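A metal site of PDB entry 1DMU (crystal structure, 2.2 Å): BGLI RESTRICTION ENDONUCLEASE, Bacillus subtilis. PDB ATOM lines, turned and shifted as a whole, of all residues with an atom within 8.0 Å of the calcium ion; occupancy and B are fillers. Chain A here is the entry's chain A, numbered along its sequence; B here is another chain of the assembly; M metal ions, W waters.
The side-chain amide oxygen (OE1) of Gln 100 of chain A lies within hydrogen-bond range of the guanidinium group (NH1) of Arg 96 of chain A (2.9 Å). The backbone carbonyl oxygen (O) of Arg 96 of chain A sits at hydrogen-bond distance from the side-chain hydroxyl (OG) of Ser 99.
Gln 100 of chain A touches the calcium ion. Glu 102 touches the calcium ion. Five residues have an atom within 4 Å of the calcium ion: Ser 99, Gln 100 of chain A, Arg 101, Glu 102 and Ile 104.
The calcium ion is bound by O of Arg 101 (2.2 Å), O of Ile 104 (2.4 Å), O of Ser 99 (2.5 Å), water W1 (2.5 Å), water W3 (2.6 Å) and water W2 (2.7 Å). The calcium ion has six donor atoms within binding distance.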
ATOM      1  N   ARG A  96       9.501   5.643   5.655  1.00  0.00           N
ATOM      2  CA  ARG A  96       8.388   5.061   6.401  1.00  0.00           C
ATOM      3  C   ARG A  96       7.765   6.054   7.393  1.00  0.00           C
ATOM      4  O   ARG A  96       6.534   6.163   7.485  1.00  0.00           O
ATOM      5  CB  ARG A  96       8.838   3.810   7.171  1.00  0.00           C
ATOM      6  CG  ARG A  96       7.739   3.271   8.123  1.00  0.00           C
ATOM      7  CD  ARG A  96       8.174   2.000   8.877  1.00  0.00           C
ATOM      8  NE  ARG A  96       9.323   2.204   9.745  1.00  0.00           N
ATOM      9  CZ  ARG A  96       9.286   2.822  10.929  1.00  0.00           C
ATOM     10  NH1 ARG A  96       8.142   3.323  11.390  1.00  0.00           N
ATOM     11  NH2 ARG A  96      10.391   2.946  11.644  1.00  0.00           N
ATOM     12  N   LEU A  97       8.601   6.771   8.129  1.00  0.00           N
ATOM     13  CA  LEU A  97       8.092   7.726   9.101  1.00  0.00           C
ATOM     14  C   LEU A  97       7.330   8.867   8.455  1.00  0.00           C
ATOM     15  O   LEU A  97       6.382   9.376   9.039  1.00  0.00           O
ATOM     16  CB  LEU A  97       9.237   8.273   9.953  1.00  0.00           C
ATOM     17  CG  LEU A  97       9.913   7.219  10.843  1.00  0.00           C
ATOM     18  CD1 LEU A  97      11.228   7.770  11.372  1.00  0.00           C
ATOM     19  CD2 LEU A  97       8.987   6.859  11.984  1.00  0.00           C
ATOM     20  N   VAL A  98       7.738   9.292   7.259  1.00  0.00           N
ATOM     21  CA  VAL A  98       7.046  10.373   6.587  1.00  0.00           C
ATOM     22  C   VAL A  98       5.639   9.898   6.209  1.00  0.00           C
ATOM     23  O   VAL A  98       4.647  10.615   6.396  1.00  0.00           O
ATOM     24  CB  VAL A  98       7.816  10.846   5.300  1.00  0.00           C
ATOM     25  CG1 VAL A  98       6.888  11.565   4.337  1.00  0.00           C
ATOM     26  CG2 VAL A  98       8.966  11.777   5.693  1.00  0.00           C
ATOM     27  N   SER A  99       5.545   8.672   5.689  1.00  0.00           N
ATOM     28  CA  SER A  99       4.251   8.109   5.282  1.00  0.00           C
ATOM     29  C   SER A  99       3.316   7.881   6.469  1.00  0.00           C
ATOM     30  O   SER A  99       2.099   7.841   6.315  1.00  0.00           O
ATOM     31  CB  SER A  99       4.460   6.789   4.533  1.00  0.00           C
ATOM     32  OG  SER A  99       4.649   5.692   5.403  1.00  0.00           O
ATOM     33  N   GLN A 100       3.887   7.734   7.667  1.00  0.00           N
ATOM     34  CA  GLN A 100       3.102   7.516   8.872  1.00  0.00           C
ATOM     35  C   GLN A 100       2.559   8.841   9.404  1.00  0.00           C
ATOM     36  O   GLN A 100       1.768   8.853  10.332  1.00  0.00           O
ATOM     37  CB  GLN A 100       3.950   6.826   9.943  1.00  0.00           C
ATOM     38  CG  GLN A 100       4.515   5.489   9.516  1.00  0.00           C
ATOM     39  CD  GLN A 100       5.175   4.721  10.652  1.00  0.00           C
ATOM     40  OE1 GLN A 100       5.355   3.508  10.563  1.00  0.00           O
ATOM     41  NE2 GLN A 100       5.546   5.422  11.714  1.00  0.00           N
ATOM     42  N   ARG A 101       2.989   9.949   8.823  1.00  0.00           N
ATOM     43  CA  ARG A 101       2.466  11.224   9.270  1.00  0.00           C
ATOM     44  C   ARG A 101       0.987  11.182   8.934  1.00  0.00           C
ATOM     45  O   ARG A 101       0.583  10.727   7.854  1.00  0.00           O
ATOM     46  CB  ARG A 101       3.190  12.359   8.557  1.00  0.00           C
ATOM     47  CG  ARG A 101       4.595  12.527   9.077  1.00  0.00           C
ATOM     48  CD  ARG A 101       4.621  13.293  10.404  1.00  0.00           C
ATOM     49  NE  ARG A 101       4.314  14.693  10.160  1.00  0.00           N
ATOM     50  CZ  ARG A 101       5.102  15.717  10.471  1.00  0.00           C
ATOM     51  NH1 ARG A 101       6.271  15.535  11.069  1.00  0.00           N
ATOM     52  NH2 ARG A 101       4.715  16.938  10.136  1.00  0.00           N
ATOM     53  N   GLU A 102       0.178  11.625   9.876  1.00  0.00           N
ATOM     54  CA  GLU A 102      -1.272  11.611   9.770  1.00  0.00           C
ATOM     55  C   GLU A 102      -1.846  12.059   8.425  1.00  0.00           C
ATOM     56  O   GLU A 102      -2.604  11.321   7.771  1.00  0.00           O
ATOM     57  CB  GLU A 102      -1.876  12.451  10.897  1.00  0.00           C
ATOM     58  N   ASP A 103      -1.473  13.255   8.024  1.00  0.00           N
ATOM     59  CA  ASP A 103      -1.970  13.906   6.814  1.00  0.00           C
ATOM     60  C   ASP A 103      -1.247  13.606   5.500  1.00  0.00           C
ATOM     61  O   ASP A 103      -1.561  14.191   4.463  1.00  0.00           O
ATOM     62  CB  ASP A 103      -1.857  15.393   7.032  1.00  0.00           C
ATOM     63  CG  ASP A 103      -0.415  15.784   7.374  1.00  0.00           C
ATOM     64  OD1 ASP A 103       0.146  15.191   8.344  1.00  0.00           O
ATOM     65  OD2 ASP A 103       0.144  16.669   6.677  1.00  0.00           O
ATOM     66  N   ILE A 104      -0.273  12.715   5.541  1.00  0.00           N
ATOM     67  CA  ILE A 104       0.493  12.444   4.353  1.00  0.00           C
ATOM     68  C   ILE A 104       0.225  11.079   3.723  1.00  0.00           C
ATOM     69  O   ILE A 104       0.128  10.075   4.424  1.00  0.00           O
ATOM     70  CB  ILE A 104       2.017  12.614   4.655  1.00  0.00           C
ATOM     71  CG1 ILE A 104       2.298  14.055   5.091  1.00  0.00           C
ATOM     72  CG2 ILE A 104       2.872  12.259   3.437  1.00  0.00           C
ATOM     73  CD1 ILE A 104       3.711  14.279   5.625  1.00  0.00           C
ATOM     74  N   THR A 105       0.059  11.060   2.405  1.00  0.00           N
ATOM     75  CA  THR A 105      -0.144   9.831   1.676  1.00  0.00           C
ATOM     76  C   THR A 105       1.062   9.685   0.741  1.00  0.00           C
ATOM     77  O   THR A 105       1.461  10.628   0.046  1.00  0.00           O
ATOM     78  CB  THR A 105      -1.438   9.849   0.865  1.00  0.00           C
ATOM     79  OG1 THR A 105      -2.554   9.959   1.745  1.00  0.00           O
ATOM     80  CG2 THR A 105      -1.578   8.558   0.048  1.00  0.00           C
ATOM     81  N   VAL A 106       1.627   8.489   0.724  1.00  0.00           N
ATOM     82  CA  VAL A 106       2.801   8.203  -0.083  1.00  0.00           C
ATOM     83  C   VAL A 106       2.434   7.214  -1.195  1.00  0.00           C
ATOM     84  O   VAL A 106       1.643   6.301  -0.950  1.00  0.00           O
ATOM     85  CB  VAL A 106       3.908   7.587   0.830  1.00  0.00           C
ATOM     86  CG1 VAL A 106       5.018   6.972  -0.008  1.00  0.00           C
ATOM     87  CG2 VAL A 106       4.456   8.652   1.778  1.00  0.00           C
ATOM     88  N   THR A 122       1.521  13.336  -1.114  1.00  0.00           N
ATOM     89  CA  THR A 122       0.286  14.075  -1.300  1.00  0.00           C
ATOM     90  C   THR A 122      -0.233  14.494   0.085  1.00  0.00           C
ATOM     91  O   THR A 122      -0.182  13.712   1.054  1.00  0.00           O
ATOM     92  CB  THR A 122      -0.768  13.202  -2.014  1.00  0.00           C
ATOM     93  OG1 THR A 122      -0.240  12.710  -3.245  1.00  0.00           O
ATOM     94  CG2 THR A 122      -2.037  14.005  -2.302  1.00  0.00           C
ATOM     95  N   ARG B  96       6.585  -0.797   2.968  1.00  0.00           N
ATOM     96  CA  ARG B  96       5.660   0.120   3.631  1.00  0.00           C
ATOM     97  C   ARG B  96       4.327  -0.552   3.992  1.00  0.00           C
ATOM     98  O   ARG B  96       3.814  -0.374   5.106  1.00  0.00           O
ATOM     99  CB  ARG B  96       5.374   1.344   2.748  1.00  0.00           C
ATOM    100  CG  ARG B  96       4.255   2.247   3.330  1.00  0.00           C
ATOM    101  CD  ARG B  96       3.983   3.491   2.463  1.00  0.00           C
ATOM    102  NE  ARG B  96       3.519   3.175   1.121  1.00  0.00           N
ATOM    103  CZ  ARG B  96       2.284   2.766   0.817  1.00  0.00           C
ATOM    104  NH1 ARG B  96       1.375   2.603   1.776  1.00  0.00           N
ATOM    105  NH2 ARG B  96       1.962   2.514  -0.440  1.00  0.00           N
ATOM    106  N   GLN B 100       2.434  -1.283   7.709  1.00  0.00           N
ATOM    107  CA  GLN B 100       1.116  -0.720   7.958  1.00  0.00           C
ATOM    108  C   GLN B 100       0.160  -1.798   8.463  1.00  0.00           C
ATOM    109  O   GLN B 100      -0.956  -1.497   8.854  1.00  0.00           O
ATOM    110  CB  GLN B 100       0.562  -0.078   6.684  1.00  0.00           C
ATOM    111  CG  GLN B 100       1.432   1.023   6.119  1.00  0.00           C
ATOM    112  CD  GLN B 100       0.772   1.791   4.983  1.00  0.00           C
ATOM    113  OE1 GLN B 100       1.179   2.908   4.667  1.00  0.00           O
ATOM    114  NE2 GLN B 100      -0.235   1.195   4.360  1.00  0.00           N
HETATM  115 CA    CA M   1      -0.037   9.014   6.584  1.00  0.00          CA
HETATM  116  O   HOH W   1      -0.885   7.332   8.224  1.00  0.00           O
HETATM  117  O   HOH W   2      -2.742   9.178   6.307  1.00  0.00           O
HETATM  118  O   HOH W   3      -0.606   6.792   5.421  1.00  0.00           O
